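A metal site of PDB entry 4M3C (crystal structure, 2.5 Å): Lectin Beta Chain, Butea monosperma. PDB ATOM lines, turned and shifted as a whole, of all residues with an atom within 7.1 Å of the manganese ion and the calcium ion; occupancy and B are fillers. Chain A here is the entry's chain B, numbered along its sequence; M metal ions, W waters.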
ATOM      1  N   ASP A  88      22.016  23.629   7.138  1.00  0.00           N
ATOM      2  CA  ASP A  88      20.632  24.071   7.105  1.00  0.00           C
ATOM      3  C   ASP A  88      20.503  25.603   7.264  1.00  0.00           C
ATOM      4  O   ASP A  88      19.680  26.247   6.571  1.00  0.00           O
ATOM      5  CB  ASP A  88      19.836  23.347   8.188  1.00  0.00           C
ATOM      6  CG  ASP A  88      18.978  22.195   7.620  1.00  0.00           C
ATOM      7  OD1 ASP A  88      18.113  22.441   6.747  1.00  0.00           O
ATOM      8  OD2 ASP A  88      19.120  21.046   8.119  1.00  0.00           O
ATOM      9  N   GLY A  89      21.325  26.199   8.150  1.00  0.00           N
ATOM     10  CA  GLY A  89      21.374  27.642   8.268  1.00  0.00           C
ATOM     11  C   GLY A  89      21.858  28.089   9.629  1.00  0.00           C
ATOM     12  O   GLY A  89      22.136  27.267  10.497  1.00  0.00           O
ATOM     13  N   ALA A 105      18.788  20.462  12.265  1.00  0.00           N
ATOM     14  CA  ALA A 105      18.448  20.499  10.857  1.00  0.00           C
ATOM     15  C   ALA A 105      17.493  21.713  10.595  1.00  0.00           C
ATOM     16  O   ALA A 105      17.731  22.790  11.108  1.00  0.00           O
ATOM     17  CB  ALA A 105      17.840  19.156  10.439  1.00  0.00           C
ATOM     18  N   GLY A 106      16.434  21.565   9.808  1.00  0.00           N
ATOM     19  CA  GLY A 106      15.634  22.722   9.391  1.00  0.00           C
ATOM     20  C   GLY A 106      14.979  23.542  10.489  1.00  0.00           C
ATOM     21  O   GLY A 106      14.467  24.631  10.244  1.00  0.00           O
ATOM     22  N   PHE A 107      14.993  23.021  11.704  1.00  0.00           N
ATOM     23  CA  PHE A 107      14.475  23.738  12.868  1.00  0.00           C
ATOM     24  C   PHE A 107      15.508  24.729  13.430  1.00  0.00           C
ATOM     25  O   PHE A 107      15.193  25.583  14.281  1.00  0.00           O
ATOM     26  CB  PHE A 107      14.057  22.736  13.965  1.00  0.00           C
ATOM     27  CG  PHE A 107      13.098  21.681  13.476  1.00  0.00           C
ATOM     28  CD1 PHE A 107      13.556  20.500  12.929  1.00  0.00           C
ATOM     29  CD2 PHE A 107      11.721  21.877  13.566  1.00  0.00           C
ATOM     30  CE1 PHE A 107      12.694  19.531  12.480  1.00  0.00           C
ATOM     31  CE2 PHE A 107      10.846  20.909  13.112  1.00  0.00           C
ATOM     32  CZ  PHE A 107      11.331  19.727  12.574  1.00  0.00           C
ATOM     33  N   LEU A 108      16.751  24.613  12.969  1.00  0.00           N
ATOM     34  CA  LEU A 108      17.779  25.569  13.386  1.00  0.00           C
ATOM     35  C   LEU A 108      17.864  25.702  14.934  1.00  0.00           C
ATOM     36  O   LEU A 108      18.168  26.771  15.474  1.00  0.00           O
ATOM     37  CB  LEU A 108      17.516  26.915  12.707  1.00  0.00           C
ATOM     38  CG  LEU A 108      17.308  26.902  11.191  1.00  0.00           C
ATOM     39  CD1 LEU A 108      17.232  28.310  10.595  1.00  0.00           C
ATOM     40  CD2 LEU A 108      18.428  26.168  10.487  1.00  0.00           C
ATOM     41  N   GLU A 126      16.595  34.275  10.538  1.00  0.00           N
ATOM     42  CA  GLU A 126      17.290  33.157   9.970  1.00  0.00           C
ATOM     43  C   GLU A 126      17.870  33.511   8.622  1.00  0.00           C
ATOM     44  O   GLU A 126      17.279  34.289   7.827  1.00  0.00           O
ATOM     45  CB  GLU A 126      16.358  31.970   9.790  1.00  0.00           C
ATOM     46  CG  GLU A 126      15.225  32.243   8.802  1.00  0.00           C
ATOM     47  CD  GLU A 126      14.423  30.995   8.409  1.00  0.00           C
ATOM     48  OE1 GLU A 126      14.007  30.195   9.310  1.00  0.00           O
ATOM     49  OE2 GLU A 126      14.211  30.846   7.184  1.00  0.00           O
ATOM     50  N   PHE A 127      19.028  32.892   8.397  1.00  0.00           N
ATOM     51  CA  PHE A 127      19.738  32.871   7.145  1.00  0.00           C
ATOM     52  C   PHE A 127      19.690  31.390   6.818  1.00  0.00           C
ATOM     53  O   PHE A 127      20.413  30.569   7.415  1.00  0.00           O
ATOM     54  CB  PHE A 127      21.141  33.394   7.386  1.00  0.00           C
ATOM     55  CG  PHE A 127      21.162  34.807   7.912  1.00  0.00           C
ATOM     56  CD1 PHE A 127      21.245  35.892   7.043  1.00  0.00           C
ATOM     57  CD2 PHE A 127      21.037  35.058   9.255  1.00  0.00           C
ATOM     58  CE1 PHE A 127      21.230  37.193   7.505  1.00  0.00           C
ATOM     59  CE2 PHE A 127      21.031  36.367   9.733  1.00  0.00           C
ATOM     60  CZ  PHE A 127      21.131  37.445   8.857  1.00  0.00           C
ATOM     61  N   ASP A 128      18.756  31.065   5.924  1.00  0.00           N
ATOM     62  CA  ASP A 128      18.301  29.691   5.681  1.00  0.00           C
ATOM     63  C   ASP A 128      18.693  29.165   4.304  1.00  0.00           C
ATOM     64  O   ASP A 128      18.289  29.721   3.258  1.00  0.00           O
ATOM     65  CB  ASP A 128      16.792  29.583   5.892  1.00  0.00           C
ATOM     66  CG  ASP A 128      16.252  28.199   5.566  1.00  0.00           C
ATOM     67  OD1 ASP A 128      17.038  27.334   5.164  1.00  0.00           O
ATOM     68  OD2 ASP A 128      15.035  27.964   5.683  1.00  0.00           O
ATOM     69  N   THR A 129      19.433  28.062   4.329  1.00  0.00           N
ATOM     70  CA  THR A 129      20.187  27.640   3.162  1.00  0.00           C
ATOM     71  C   THR A 129      19.694  26.372   2.502  1.00  0.00           C
ATOM     72  O   THR A 129      20.391  25.826   1.654  1.00  0.00           O
ATOM     73  CB  THR A 129      21.677  27.425   3.503  1.00  0.00           C
ATOM     74  OG1 THR A 129      21.778  26.498   4.603  1.00  0.00           O
ATOM     75  CG2 THR A 129      22.373  28.796   3.854  1.00  0.00           C
ATOM     76  N   TYR A 130      18.491  25.934   2.881  1.00  0.00           N
ATOM     77  CA  TYR A 130      17.964  24.657   2.398  1.00  0.00           C
ATOM     78  C   TYR A 130      16.432  24.547   2.497  1.00  0.00           C
ATOM     79  O   TYR A 130      15.835  24.707   3.578  1.00  0.00           O
ATOM     80  CB  TYR A 130      18.594  23.502   3.157  1.00  0.00           C
ATOM     81  CG  TYR A 130      17.960  22.163   2.841  1.00  0.00           C
ATOM     82  CD1 TYR A 130      18.463  21.367   1.799  1.00  0.00           C
ATOM     83  CD2 TYR A 130      16.863  21.693   3.562  1.00  0.00           C
ATOM     84  CE1 TYR A 130      17.903  20.156   1.506  1.00  0.00           C
ATOM     85  CE2 TYR A 130      16.292  20.466   3.257  1.00  0.00           C
ATOM     86  CZ  TYR A 130      16.826  19.707   2.229  1.00  0.00           C
ATOM     87  OH  TYR A 130      16.289  18.490   1.912  1.00  0.00           O
ATOM     88  N   GLU A 131      15.818  24.222   1.372  1.00  0.00           N
ATOM     89  CA  GLU A 131      14.390  24.357   1.257  1.00  0.00           C
ATOM     90  C   GLU A 131      13.667  23.208   1.902  1.00  0.00           C
ATOM     91  O   GLU A 131      13.751  22.086   1.428  1.00  0.00           O
ATOM     92  CB  GLU A 131      13.953  24.487  -0.200  1.00  0.00           C
ATOM     93  CG  GLU A 131      12.510  24.947  -0.281  1.00  0.00           C
ATOM     94  CD  GLU A 131      11.821  24.703  -1.612  1.00  0.00           C
ATOM     95  OE1 GLU A 131      12.328  23.977  -2.489  1.00  0.00           O
ATOM     96  OE2 GLU A 131      10.731  25.263  -1.778  1.00  0.00           O
ATOM     97  N   ASN A 132      12.959  23.502   3.000  1.00  0.00           N
ATOM     98  CA  ASN A 132      12.035  22.543   3.590  1.00  0.00           C
ATOM     99  C   ASN A 132      10.629  22.914   3.100  1.00  0.00           C
ATOM    100  O   ASN A 132      10.013  23.868   3.546  1.00  0.00           O
ATOM    101  CB  ASN A 132      12.071  22.529   5.110  1.00  0.00           C
ATOM    102  CG  ASN A 132      13.463  22.405   5.682  1.00  0.00           C
ATOM    103  OD1 ASN A 132      13.856  21.317   6.138  1.00  0.00           O
ATOM    104  ND2 ASN A 132      14.218  23.530   5.721  1.00  0.00           N
ATOM    105  N   PHE A 135       7.922  23.537   5.723  1.00  0.00           N
ATOM    106  CA  PHE A 135       7.929  24.860   6.413  1.00  0.00           C
ATOM    107  C   PHE A 135       7.578  25.996   5.481  1.00  0.00           C
ATOM    108  O   PHE A 135       7.703  27.154   5.837  1.00  0.00           O
ATOM    109  CB  PHE A 135       9.253  25.179   7.110  1.00  0.00           C
ATOM    110  CG  PHE A 135       9.826  24.044   7.907  1.00  0.00           C
ATOM    111  CD1 PHE A 135       8.991  23.058   8.456  1.00  0.00           C
ATOM    112  CD2 PHE A 135      11.209  23.959   8.115  1.00  0.00           C
ATOM    113  CE1 PHE A 135       9.527  21.991   9.155  1.00  0.00           C
ATOM    114  CE2 PHE A 135      11.751  22.894   8.822  1.00  0.00           C
ATOM    115  CZ  PHE A 135      10.909  21.918   9.345  1.00  0.00           C
ATOM    116  N   LEU A 136       7.131  25.645   4.280  1.00  0.00           N
ATOM    117  CA  LEU A 136       6.877  26.609   3.219  1.00  0.00           C
ATOM    118  C   LEU A 136       8.097  27.501   2.907  1.00  0.00           C
ATOM    119  O   LEU A 136       7.926  28.661   2.522  1.00  0.00           O
ATOM    120  CB  LEU A 136       5.582  27.406   3.470  1.00  0.00           C
ATOM    121  CG  LEU A 136       4.323  26.491   3.626  1.00  0.00           C
ATOM    122  CD1 LEU A 136       3.479  26.786   4.869  1.00  0.00           C
ATOM    123  CD2 LEU A 136       3.464  26.360   2.358  1.00  0.00           C
ATOM    124  N   ASP A 137       9.315  26.950   3.066  1.00  0.00           N
ATOM    125  CA  ASP A 137      10.537  27.637   2.598  1.00  0.00           C
ATOM    126  C   ASP A 137      10.384  27.988   1.105  1.00  0.00           C
ATOM    127  O   ASP A 137       9.792  27.203   0.344  1.00  0.00           O
ATOM    128  CB  ASP A 137      11.815  26.779   2.787  1.00  0.00           C
ATOM    129  CG  ASP A 137      12.457  26.935   4.176  1.00  0.00           C
ATOM    130  OD1 ASP A 137      12.183  27.861   4.943  1.00  0.00           O
ATOM    131  OD2 ASP A 137      13.308  26.096   4.515  1.00  0.00           O
ATOM    132  N   PRO A 138      10.851  29.176   0.698  1.00  0.00           N
ATOM    133  CA  PRO A 138      10.832  29.556  -0.725  1.00  0.00           C
ATOM    134  C   PRO A 138      11.881  28.778  -1.529  1.00  0.00           C
ATOM    135  O   PRO A 138      12.825  28.277  -0.937  1.00  0.00           O
ATOM    136  CB  PRO A 138      11.143  31.061  -0.707  1.00  0.00           C
ATOM    137  CG  PRO A 138      11.685  31.362   0.661  1.00  0.00           C
ATOM    138  CD  PRO A 138      11.270  30.277   1.594  1.00  0.00           C
ATOM    139  N   ASP A 140      14.447  29.338  -2.955  1.00  0.00           N
ATOM    140  CA  ASP A 140      15.760  29.971  -3.038  1.00  0.00           C
ATOM    141  C   ASP A 140      16.314  30.039  -1.606  1.00  0.00           C
ATOM    142  O   ASP A 140      15.567  29.899  -0.648  1.00  0.00           O
ATOM    143  CB  ASP A 140      15.738  31.333  -3.821  1.00  0.00           C
ATOM    144  CG  ASP A 140      14.580  32.319  -3.401  1.00  0.00           C
ATOM    145  OD1 ASP A 140      14.771  33.182  -2.482  1.00  0.00           O
ATOM    146  OD2 ASP A 140      13.503  32.322  -4.070  1.00  0.00           O
ATOM    147  N   HIS A 142      17.351  31.997   1.574  1.00  0.00           N
ATOM    148  CA  HIS A 142      16.675  33.253   1.942  1.00  0.00           C
ATOM    149  C   HIS A 142      16.922  33.752   3.322  1.00  0.00           C
ATOM    150  O   HIS A 142      17.267  32.988   4.210  1.00  0.00           O
ATOM    151  CB  HIS A 142      15.186  33.047   1.821  1.00  0.00           C
ATOM    152  CG  HIS A 142      14.690  31.848   2.590  1.00  0.00           C
ATOM    153  ND1 HIS A 142      14.747  30.600   2.091  1.00  0.00           N
ATOM    154  CD2 HIS A 142      14.145  31.737   3.866  1.00  0.00           C
ATOM    155  CE1 HIS A 142      14.255  29.747   2.999  1.00  0.00           C
ATOM    156  NE2 HIS A 142      13.890  30.448   4.078  1.00  0.00           N
ATOM    157  N   ILE A 143      16.687  35.045   3.518  1.00  0.00           N
ATOM    158  CA  ILE A 143      16.598  35.646   4.854  1.00  0.00           C
ATOM    159  C   ILE A 143      15.145  35.627   5.278  1.00  0.00           C
ATOM    160  O   ILE A 143      14.238  35.939   4.488  1.00  0.00           O
ATOM    161  CB  ILE A 143      17.120  37.090   4.911  1.00  0.00           C
ATOM    162  CG1 ILE A 143      18.576  37.126   4.477  1.00  0.00           C
ATOM    163  CG2 ILE A 143      16.966  37.646   6.331  1.00  0.00           C
ATOM    164  CD1 ILE A 143      19.174  38.520   4.347  1.00  0.00           C
ATOM    165  N   GLY A 144      14.919  35.198   6.520  1.00  0.00           N
ATOM    166  CA  GLY A 144      13.556  35.022   7.064  1.00  0.00           C
ATOM    167  C   GLY A 144      13.419  35.571   8.477  1.00  0.00           C
ATOM    168  O   GLY A 144      14.365  35.513   9.277  1.00  0.00           O
ATOM    169  N   ASP A 146      11.348  34.857  11.827  1.00  0.00           N
ATOM    170  CA  ASP A 146      10.539  33.761  12.436  1.00  0.00           C
ATOM    171  C   ASP A 146      10.049  34.179  13.798  1.00  0.00           C
ATOM    172  O   ASP A 146      10.820  34.539  14.685  1.00  0.00           O
ATOM    173  CB  ASP A 146      11.314  32.448  12.614  1.00  0.00           C
ATOM    174  CG  ASP A 146      12.132  32.049  11.384  1.00  0.00           C
ATOM    175  OD1 ASP A 146      11.717  32.426  10.265  1.00  0.00           O
ATOM    176  OD2 ASP A 146      13.192  31.381  11.555  1.00  0.00           O
ATOM    177  N   ILE A 150       9.139  28.199  12.685  1.00  0.00           N
ATOM    178  CA  ILE A 150      10.173  28.096  11.653  1.00  0.00           C
ATOM    179  C   ILE A 150       9.595  28.508  10.302  1.00  0.00           C
ATOM    180  O   ILE A 150      10.329  28.679   9.312  1.00  0.00           O
ATOM    181  CB  ILE A 150      10.693  26.651  11.543  1.00  0.00           C
ATOM    182  CG1 ILE A 150      11.993  26.587  10.722  1.00  0.00           C
ATOM    183  CG2 ILE A 150       9.619  25.762  10.922  1.00  0.00           C
ATOM    184  CD1 ILE A 150      13.205  27.275  11.316  1.00  0.00           C
ATOM    185  N   LYS A 151       8.289  28.666  10.265  1.00  0.00           N
ATOM    186  CA  LYS A 151       7.596  29.172   9.104  1.00  0.00           C
ATOM    187  C   LYS A 151       7.576  30.686   9.181  1.00  0.00           C
ATOM    188  O   LYS A 151       6.751  31.268   9.851  1.00  0.00           O
ATOM    189  CB  LYS A 151       6.176  28.577   9.059  1.00  0.00           C
ATOM    190  CG  LYS A 151       5.526  28.666   7.688  1.00  0.00           C
ATOM    191  CD  LYS A 151       4.550  29.830   7.537  1.00  0.00           C
ATOM    192  CE  LYS A 151       3.431  29.453   6.554  1.00  0.00           C
ATOM    193  NZ  LYS A 151       3.117  30.521   5.556  1.00  0.00           N
ATOM    194  N   SER A 152       8.504  31.321   8.474  1.00  0.00           N
ATOM    195  CA  SER A 152       8.725  32.756   8.567  1.00  0.00           C
ATOM    196  C   SER A 152       7.502  33.589   8.229  1.00  0.00           C
ATOM    197  O   SER A 152       6.828  33.287   7.268  1.00  0.00           O
ATOM    198  CB  SER A 152       9.865  33.094   7.605  1.00  0.00           C
ATOM    199  OG  SER A 152      10.971  32.236   7.824  1.00  0.00           O
ATOM    200  N   THR A 155      10.010  36.705   4.204  1.00  0.00           N
ATOM    201  CA  THR A 155      11.288  36.294   3.645  1.00  0.00           C
ATOM    202  C   THR A 155      11.761  37.127   2.430  1.00  0.00           C
ATOM    203  O   THR A 155      10.934  37.718   1.726  1.00  0.00           O
ATOM    204  CB  THR A 155      11.262  34.814   3.203  1.00  0.00           C
ATOM    205  OG1 THR A 155      10.352  34.689   2.114  1.00  0.00           O
ATOM    206  CG2 THR A 155      10.803  33.895   4.311  1.00  0.00           C
HETATM  207 MN    MN M   1      13.419  29.336   5.988  1.00  0.00          MN
HETATM  208 CA    CA M   2      15.292  25.609   5.753  1.00  0.00          CA
HETATM  209  O   HOH W   1      11.301  30.517   5.968  1.00  0.00           O
HETATM  210  O   HOH W   2      12.547  28.252   7.825  1.00  0.00           O
HETATM  211  O   HOH W   3      16.977  24.796   6.430  1.00  0.00           O
HETATM  212  O   HOH W   4      14.048  25.732   7.431  1.00  0.00           O
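The side-chain carboxylate (OE1) of Glu 126 sits close to the side-chain carboxylate (OD2) of Asp 146, at 2.7 Å.
N of Glu 126 sits at hydrogen-bond distance from O of Gly 144, 2.8 Å away.
A ring nitrogen (ND1) of His 142 is in hydrogen-bond range of the backbone carbonyl oxygen of Asp 140, at 2.9 Å.
Within 4 Å of the manganese ion: Glu 126, Asp 128, Asp 137 and His 142.
The nearest printed residue that does not touch the manganese ion is Ser 152 (4.2 Å).
Of the 26 residues printed, 4 come within 4 Å of the calcium ion.
Along chain A the residues within 4 Å of the calcium ion span positions 128 to 137.
The nearest printed residue that does not touch the calcium ion is Asp 88 (4.4 Å).
The manganese ion is bound by OE2 of Glu 126 (2.1 Å), OD2 of Asp 128 (2.1 Å), OD1 of Asp 137 (2.2 Å), NE2 of His 142 (2.3 Å), water W2 (2.3 Å) and water W1 (2.4 Å).
The calcium ion is bound by water W3 (2.0 Å), water W4 (2.1 Å), the side-chain amide nitrogen (ND2) of Asn 132 (2.3 Å), the side-chain carboxylate (OD2) of Asp 128 (2.4 Å), the side-chain carboxylate (OD2) of Asp 137 (2.4 Å), the backbone carbonyl oxygen (O) of Tyr 130 (2.4 Å) and the side-chain carboxylate (OD1) of Asp 128 (2.5 Å).
The calcium ion has seven donor atoms within binding distance.
Water W2 bridges the backbone carbonyl oxygen (O) of Ile 150 (2.7 Å) and the side-chain carboxylate (OE1) of Glu 126 (2.8 Å).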
